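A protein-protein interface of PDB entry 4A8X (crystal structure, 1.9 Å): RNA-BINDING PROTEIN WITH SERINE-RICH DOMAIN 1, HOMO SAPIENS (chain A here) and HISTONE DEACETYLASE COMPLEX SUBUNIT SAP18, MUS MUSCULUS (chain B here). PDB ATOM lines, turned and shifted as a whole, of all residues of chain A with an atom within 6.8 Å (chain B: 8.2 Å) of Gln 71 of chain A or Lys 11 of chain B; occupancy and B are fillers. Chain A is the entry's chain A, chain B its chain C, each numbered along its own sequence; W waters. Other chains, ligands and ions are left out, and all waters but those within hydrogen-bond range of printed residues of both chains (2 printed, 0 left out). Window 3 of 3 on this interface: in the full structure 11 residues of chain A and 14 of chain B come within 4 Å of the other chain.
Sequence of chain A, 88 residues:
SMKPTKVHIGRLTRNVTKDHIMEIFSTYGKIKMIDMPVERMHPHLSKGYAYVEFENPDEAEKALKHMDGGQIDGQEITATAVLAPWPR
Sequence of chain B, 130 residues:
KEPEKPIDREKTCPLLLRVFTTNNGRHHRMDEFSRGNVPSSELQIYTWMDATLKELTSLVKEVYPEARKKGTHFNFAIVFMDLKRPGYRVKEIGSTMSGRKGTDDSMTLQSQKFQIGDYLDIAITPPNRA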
ATOM      1  N   ILE A  24      15.535 -12.663  20.229  1.00  0.00           N
ATOM      2  CA  ILE A  24      16.156 -12.195  19.015  1.00  0.00           C
ATOM      3  C   ILE A  24      17.269 -11.158  19.321  1.00  0.00           C
ATOM      4  O   ILE A  24      18.370 -11.238  18.790  1.00  0.00           O
ATOM      5  CB  ILE A  24      15.070 -11.586  18.065  1.00  0.00           C
ATOM      6  CG1 ILE A  24      14.223 -12.712  17.450  1.00  0.00           C
ATOM      7  CG2 ILE A  24      15.702 -10.734  17.005  1.00  0.00           C
ATOM      8  CD1 ILE A  24      12.921 -12.199  16.775  1.00  0.00           C
ATOM      9  N   HIS A  66      22.624  -4.604  12.483  1.00  0.00           N
ATOM     10  CA  HIS A  66      22.082  -5.857  11.936  1.00  0.00           C
ATOM     11  C   HIS A  66      20.567  -5.898  11.740  1.00  0.00           C
ATOM     12  O   HIS A  66      20.076  -6.720  10.971  1.00  0.00           O
ATOM     13  CB  HIS A  66      22.502  -7.046  12.809  1.00  0.00           C
ATOM     14  CG  HIS A  66      23.982  -7.281  12.810  1.00  0.00           C
ATOM     15  ND1 HIS A  66      24.873  -6.368  13.328  1.00  0.00           N
ATOM     16  CD2 HIS A  66      24.725  -8.296  12.314  1.00  0.00           C
ATOM     17  CE1 HIS A  66      26.110  -6.820  13.166  1.00  0.00           C
ATOM     18  NE2 HIS A  66      26.044  -7.986  12.557  1.00  0.00           N
ATOM     19  N   MET A  67      19.810  -5.056  12.429  1.00  0.00           N
ATOM     20  CA  MET A  67      18.354  -5.248  12.427  1.00  0.00           C
ATOM     21  C   MET A  67      17.487  -4.066  11.959  1.00  0.00           C
ATOM     22  O   MET A  67      16.285  -4.229  11.793  1.00  0.00           O
ATOM     23  CB  MET A  67      17.886  -5.718  13.804  1.00  0.00           C
ATOM     24  CG  MET A  67      18.204  -7.186  14.081  1.00  0.00           C
ATOM     25  SD  MET A  67      17.485  -8.400  12.918  1.00  0.00           S
ATOM     26  CE  MET A  67      15.798  -8.566  13.567  1.00  0.00           C
ATOM     27  N   GLY A  69      15.952  -2.573   9.250  1.00  0.00           N
ATOM     28  CA  GLY A  69      15.813  -3.166   7.926  1.00  0.00           C
ATOM     29  C   GLY A  69      15.867  -4.676   7.888  1.00  0.00           C
ATOM     30  O   GLY A  69      15.735  -5.275   6.813  1.00  0.00           O
ATOM     31  N   GLY A  70      16.054  -5.301   9.058  1.00  0.00           N
ATOM     32  CA  GLY A  70      16.040  -6.748   9.190  1.00  0.00           C
ATOM     33  C   GLY A  70      14.570  -7.199   9.147  1.00  0.00           C
ATOM     34  O   GLY A  70      13.657  -6.381   8.889  1.00  0.00           O
ATOM     35  N   GLN A  71      14.352  -8.482   9.345  1.00  0.00           N
ATOM     36  CA  GLN A  71      13.008  -9.064   9.262  1.00  0.00           C
ATOM     37  C   GLN A  71      12.646  -9.847  10.500  1.00  0.00           C
ATOM     38  O   GLN A  71      13.473 -10.580  11.024  1.00  0.00           O
ATOM     39  CB  GLN A  71      12.910 -10.015   8.061  1.00  0.00           C
ATOM     40  CG  GLN A  71      13.093  -9.334   6.719  1.00  0.00           C
ATOM     41  CD  GLN A  71      13.225 -10.346   5.604  1.00  0.00           C
ATOM     42  OE1 GLN A  71      12.246 -10.974   5.218  1.00  0.00           O
ATOM     43  NE2 GLN A  71      14.448 -10.540   5.103  1.00  0.00           N
ATOM     44  N   ILE A  72      11.394  -9.711  10.947  1.00  0.00           N
ATOM     45  CA  ILE A  72      10.846 -10.515  12.036  1.00  0.00           C
ATOM     46  C   ILE A  72       9.416 -10.953  11.664  1.00  0.00           C
ATOM     47  O   ILE A  72       8.581 -10.116  11.284  1.00  0.00           O
ATOM     48  CB  ILE A  72      10.842  -9.766  13.388  1.00  0.00           C
ATOM     49  CG1 ILE A  72      12.250  -9.256  13.802  1.00  0.00           C
ATOM     50  CG2 ILE A  72      10.224 -10.700  14.493  1.00  0.00           C
ATOM     51  CD1 ILE A  72      12.322  -8.555  15.206  1.00  0.00           C
ATOM     52  N   ASP A  73       9.173 -12.250  11.755  1.00  0.00           N
ATOM     53  CA  ASP A  73       7.925 -12.888  11.327  1.00  0.00           C
ATOM     54  C   ASP A  73       7.443 -12.429   9.961  1.00  0.00           C
ATOM     55  O   ASP A  73       6.265 -12.051   9.806  1.00  0.00           O
ATOM     56  CB  ASP A  73       6.809 -12.652  12.362  1.00  0.00           C
ATOM     57  CG  ASP A  73       5.581 -13.481  12.087  1.00  0.00           C
ATOM     58  OD1 ASP A  73       5.710 -14.612  11.557  1.00  0.00           O
ATOM     59  OD2 ASP A  73       4.467 -12.982  12.401  1.00  0.00           O
ATOM     60  N   GLY A  74       8.354 -12.415   8.984  1.00  0.00           N
ATOM     61  CA  GLY A  74       8.009 -12.197   7.595  1.00  0.00           C
ATOM     62  C   GLY A  74       7.800 -10.752   7.223  1.00  0.00           C
ATOM     63  O   GLY A  74       7.322 -10.453   6.139  1.00  0.00           O
ATOM     64  N   GLN A  75       8.148  -9.854   8.130  1.00  0.00           N
ATOM     65  CA  GLN A  75       7.946  -8.436   7.923  1.00  0.00           C
ATOM     66  C   GLN A  75       9.236  -7.657   8.217  1.00  0.00           C
ATOM     67  O   GLN A  75       9.934  -7.909   9.204  1.00  0.00           O
ATOM     68  CB  GLN A  75       6.801  -7.932   8.831  1.00  0.00           C
ATOM     69  CG  GLN A  75       6.397  -6.492   8.575  1.00  0.00           C
ATOM     70  CD  GLN A  75       4.982  -6.237   9.023  1.00  0.00           C
ATOM     71  OE1 GLN A  75       4.019  -6.610   8.329  1.00  0.00           O
ATOM     72  NE2 GLN A  75       4.835  -5.653  10.222  1.00  0.00           N
ATOM     73  N   GLU A  76       9.556  -6.708   7.349  1.00  0.00           N
ATOM     74  CA  GLU A  76      10.688  -5.822   7.577  1.00  0.00           C
ATOM     75  C   GLU A  76      10.441  -4.861   8.767  1.00  0.00           C
ATOM     76  O   GLU A  76       9.358  -4.284   8.908  1.00  0.00           O
ATOM     77  CB  GLU A  76      11.036  -5.076   6.305  1.00  0.00           C
ATOM     78  CG  GLU A  76      12.244  -4.158   6.438  1.00  0.00           C
ATOM     79  CD  GLU A  76      12.717  -3.546   5.113  1.00  0.00           C
ATOM     80  OE1 GLU A  76      12.598  -4.206   4.043  1.00  0.00           O
ATOM     81  OE2 GLU A  76      13.221  -2.401   5.167  1.00  0.00           O
ATOM     82  N   ILE A  77      11.434  -4.740   9.658  1.00  0.00           N
ATOM     83  CA  ILE A  77      11.270  -3.931  10.889  1.00  0.00           C
ATOM     84  C   ILE A  77      12.200  -2.713  10.834  1.00  0.00           C
ATOM     85  O   ILE A  77      13.097  -2.645  10.001  1.00  0.00           O
ATOM     86  CB  ILE A  77      11.624  -4.716  12.192  1.00  0.00           C
ATOM     87  CG1 ILE A  77      13.092  -5.143  12.161  1.00  0.00           C
ATOM     88  CG2 ILE A  77      10.711  -5.959  12.396  1.00  0.00           C
ATOM     89  CD1 ILE A  77      13.678  -5.338  13.546  1.00  0.00           C
ATOM     90  N   ILE B   7       8.058 -11.074  -4.405  1.00  0.00           N
ATOM     91  CA  ILE B   7       8.614 -11.698  -3.213  1.00  0.00           C
ATOM     92  C   ILE B   7       9.549 -12.839  -3.606  1.00  0.00           C
ATOM     93  O   ILE B   7       9.144 -13.787  -4.286  1.00  0.00           O
ATOM     94  CB  ILE B   7       7.498 -12.191  -2.272  1.00  0.00           C
ATOM     95  CG1 ILE B   7       6.690 -11.006  -1.730  1.00  0.00           C
ATOM     96  CG2 ILE B   7       8.091 -12.995  -1.096  1.00  0.00           C
ATOM     97  CD1 ILE B   7       5.352 -11.387  -1.139  1.00  0.00           C
ATOM     98  N   ASP B   8      10.808 -12.711  -3.190  1.00  0.00           N
ATOM     99  CA  ASP B   8      11.821 -13.766  -3.321  1.00  0.00           C
ATOM    100  C   ASP B   8      11.817 -14.570  -2.050  1.00  0.00           C
ATOM    101  O   ASP B   8      12.275 -14.115  -1.004  1.00  0.00           O
ATOM    102  CB  ASP B   8      13.220 -13.166  -3.564  1.00  0.00           C
ATOM    103  CG  ASP B   8      14.310 -14.229  -3.774  1.00  0.00           C
ATOM    104  OD1 ASP B   8      14.200 -15.378  -3.285  1.00  0.00           O
ATOM    105  OD2 ASP B   8      15.309 -13.902  -4.436  1.00  0.00           O
ATOM    106  N   ARG B   9      11.279 -15.781  -2.137  1.00  0.00           N
ATOM    107  CA  ARG B   9      11.089 -16.612  -0.964  1.00  0.00           C
ATOM    108  C   ARG B   9      12.353 -17.220  -0.369  1.00  0.00           C
ATOM    109  O   ARG B   9      12.296 -17.856   0.682  1.00  0.00           O
ATOM    110  CB  ARG B   9      10.074 -17.711  -1.265  1.00  0.00           C
ATOM    111  CG  ARG B   9       8.664 -17.159  -1.563  1.00  0.00           C
ATOM    112  CD  ARG B   9       7.659 -18.273  -1.879  1.00  0.00           C
ATOM    113  NE  ARG B   9       6.300 -17.739  -2.042  1.00  0.00           N
ATOM    114  CZ  ARG B   9       5.194 -18.470  -1.961  1.00  0.00           C
ATOM    115  NH1 ARG B   9       5.287 -19.762  -1.730  1.00  0.00           N
ATOM    116  NH2 ARG B   9       3.996 -17.912  -2.134  1.00  0.00           N
ATOM    117  N   GLU B  10      13.485 -16.988  -1.000  1.00  0.00           N
ATOM    118  CA  GLU B  10      14.770 -17.332  -0.413  1.00  0.00           C
ATOM    119  C   GLU B  10      15.392 -16.165   0.355  1.00  0.00           C
ATOM    120  O   GLU B  10      16.305 -16.361   1.148  1.00  0.00           O
ATOM    121  CB  GLU B  10      15.736 -17.815  -1.501  1.00  0.00           C
ATOM    122  CG  GLU B  10      15.349 -19.158  -2.084  1.00  0.00           C
ATOM    123  CD  GLU B  10      16.567 -20.007  -2.457  1.00  0.00           C
ATOM    124  OE1 GLU B  10      17.650 -19.427  -2.756  1.00  0.00           O
ATOM    125  OE2 GLU B  10      16.439 -21.259  -2.432  1.00  0.00           O
ATOM    126  N   LYS B  11      14.901 -14.950   0.128  1.00  0.00           N
ATOM    127  CA  LYS B  11      15.455 -13.767   0.758  1.00  0.00           C
ATOM    128  C   LYS B  11      14.509 -13.152   1.782  1.00  0.00           C
ATOM    129  O   LYS B  11      14.948 -12.475   2.709  1.00  0.00           O
ATOM    130  CB  LYS B  11      15.773 -12.707  -0.291  1.00  0.00           C
ATOM    131  CG  LYS B  11      16.792 -13.145  -1.358  1.00  0.00           C
ATOM    132  CD  LYS B  11      18.192 -13.251  -0.786  1.00  0.00           C
ATOM    133  CE  LYS B  11      19.229 -13.548  -1.875  1.00  0.00           C
ATOM    134  NZ  LYS B  11      19.306 -12.464  -2.909  1.00  0.00           N
ATOM    135  N   THR B  12      13.215 -13.349   1.586  1.00  0.00           N
ATOM    136  CA  THR B  12      12.206 -12.839   2.520  1.00  0.00           C
ATOM    137  C   THR B  12      11.768 -13.952   3.437  1.00  0.00           C
ATOM    138  O   THR B  12      11.341 -15.006   2.978  1.00  0.00           O
ATOM    139  CB  THR B  12      10.993 -12.329   1.769  1.00  0.00           C
ATOM    140  OG1 THR B  12      11.389 -11.186   0.990  1.00  0.00           O
ATOM    141  CG2 THR B  12       9.851 -11.943   2.754  1.00  0.00           C
ATOM    142  N   CYS B  13      11.890 -13.758   4.744  1.00  0.00           N
ATOM    143  CA  CYS B  13      11.518 -14.849   5.619  1.00  0.00           C
ATOM    144  C   CYS B  13       9.976 -14.985   5.672  1.00  0.00           C
ATOM    145  O   CYS B  13       9.240 -14.035   5.457  1.00  0.00           O
ATOM    146  CB  CYS B  13      12.216 -14.776   6.984  1.00  0.00           C
ATOM    147  SG  CYS B  13      11.362 -13.925   8.303  1.00  0.00           S
ATOM    148  N   PRO B  14       9.502 -16.204   5.859  1.00  0.00           N
ATOM    149  CA  PRO B  14       8.055 -16.417   5.842  1.00  0.00           C
ATOM    150  C   PRO B  14       7.362 -15.900   7.095  1.00  0.00           C
ATOM    151  O   PRO B  14       8.003 -15.796   8.128  1.00  0.00           O
ATOM    152  CB  PRO B  14       7.943 -17.929   5.809  1.00  0.00           C
ATOM    153  CG  PRO B  14       9.137 -18.400   6.544  1.00  0.00           C
ATOM    154  CD  PRO B  14      10.234 -17.440   6.127  1.00  0.00           C
ATOM    155  N   LEU B  15       6.050 -15.675   6.995  1.00  0.00           N
ATOM    156  CA  LEU B  15       5.219 -15.237   8.102  1.00  0.00           C
ATOM    157  C   LEU B  15       4.527 -16.453   8.651  1.00  0.00           C
ATOM    158  O   LEU B  15       4.295 -17.431   7.906  1.00  0.00           O
ATOM    159  CB  LEU B  15       4.162 -14.208   7.606  1.00  0.00           C
ATOM    160  CG  LEU B  15       3.147 -14.701   6.569  1.00  0.00           C
ATOM    161  CD1 LEU B  15       1.779 -14.986   7.172  1.00  0.00           C
ATOM    162  CD2 LEU B  15       3.026 -13.730   5.374  1.00  0.00           C
ATOM    163  N   TRP B  48       3.925 -16.621   2.671  1.00  0.00           N
ATOM    164  CA  TRP B  48       4.356 -15.328   2.177  1.00  0.00           C
ATOM    165  C   TRP B  48       3.130 -14.534   1.747  1.00  0.00           C
ATOM    166  O   TRP B  48       2.084 -15.112   1.503  1.00  0.00           O
ATOM    167  CB  TRP B  48       5.331 -15.496   0.993  1.00  0.00           C
ATOM    168  CG  TRP B  48       6.668 -16.030   1.415  1.00  0.00           C
ATOM    169  CD1 TRP B  48       7.793 -15.295   1.741  1.00  0.00           C
ATOM    170  CD2 TRP B  48       7.035 -17.402   1.560  1.00  0.00           C
ATOM    171  NE1 TRP B  48       8.812 -16.133   2.096  1.00  0.00           N
ATOM    172  CE2 TRP B  48       8.383 -17.433   1.983  1.00  0.00           C
ATOM    173  CE3 TRP B  48       6.360 -18.616   1.370  1.00  0.00           C
ATOM    174  CZ2 TRP B  48       9.070 -18.637   2.217  1.00  0.00           C
ATOM    175  CZ3 TRP B  48       7.041 -19.810   1.634  1.00  0.00           C
ATOM    176  CH2 TRP B  48       8.378 -19.809   2.042  1.00  0.00           C
HETATM  177  O   HOH W   1       7.517 -16.244  10.849  1.00  0.00           O
HETATM  178  O   HOH W   2       6.696 -12.837   4.665  1.00  0.00           O
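The backbone carbonyl oxygen (O) of Lys 11 of chain B lies within hydrogen-bond range of the side-chain amide nitrogen (NE2) of Gln 71 of chain A (3.1 Å).
N of Cys 13 of chain B is in hydrogen-bond range of OE1 of Gln 71 of chain A (2.8 Å).
The backbone NH of Gly 74 of chain A is in hydrogen-bond range of the side-chain sulfur of Cys 13 of chain B (3.4 Å).
The backbone carbonyl oxygen (O) of Thr 12 of chain B is in hydrogen-bond range of the indole nitrogen (NE1) of Trp 48 of chain B.
Among the printed residues, pairs that only touch across the chains: Gln 71 of chain A with Thr 12 of chain B, Gly 74 of chain A with Pro 14 of chain B, Asp 73 of chain A with Leu 15 of chain B and Asp 73 of chain A with Pro 14 of chain B.
No residue of chain B comes within 4 Å of Gly 70 of chain A.
Of the printed residues of chain B, Asp 73 of chain A touches Pro 14 and Leu 15.
Of the printed residues of chain B, Gly 74 of chain A touches Cys 13 and Pro 14.
Gln 75 of chain A touches none of the printed residues of chain B.
Lys 11 of chain B touches just one residue of chain A: Gln 71 (3.1 Å).
Of the printed residues of chain A, Thr 12 of chain B touches Gln 71.
Printed residues of chain A within 4 Å of Cys 13 of chain B: Gln 71 (2.8 Å) and Gly 74 (3.1 Å).
Printed residues of chain A within 4 Å of Leu 15 of chain B: Asp 73.
The nearest printed residue of chain A that does not touch Lys 11 of chain B is Gly 69 of chain A (8.3 Å).
The nearest printed residue of chain A that does not touch Thr 12 of chain B is Gly 74 of chain A (4.5 Å).
Printed residues of chain B that touch a printed residue of chain A: Lys 11, Thr 12, Cys 13, Pro 14 and Leu 15.
Of the 12 printed residues of chain A, 3 touch a printed residue of chain B.
Printed residues of chain A that touch a printed residue of chain B: Gln 71, Asp 73 and Gly 74.
Among the printed residues, no Asp or Glu carboxylate lies within 4 Å of a Lys or Arg side-chain nitrogen of the other chain.
Water W1 bridges the side-chain carboxylate of Asp 73 of chain A (2.5 Å) and the backbone carbonyl oxygen of Pro 14 of chain B (2.8 Å).
Water W2 lies within hydrogen-bond range of the backbone carbonyl oxygen of Gly 74 of chain A (2.9 Å) and the backbone carbonyl oxygen of Cys 13 of chain B (2.9 Å).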
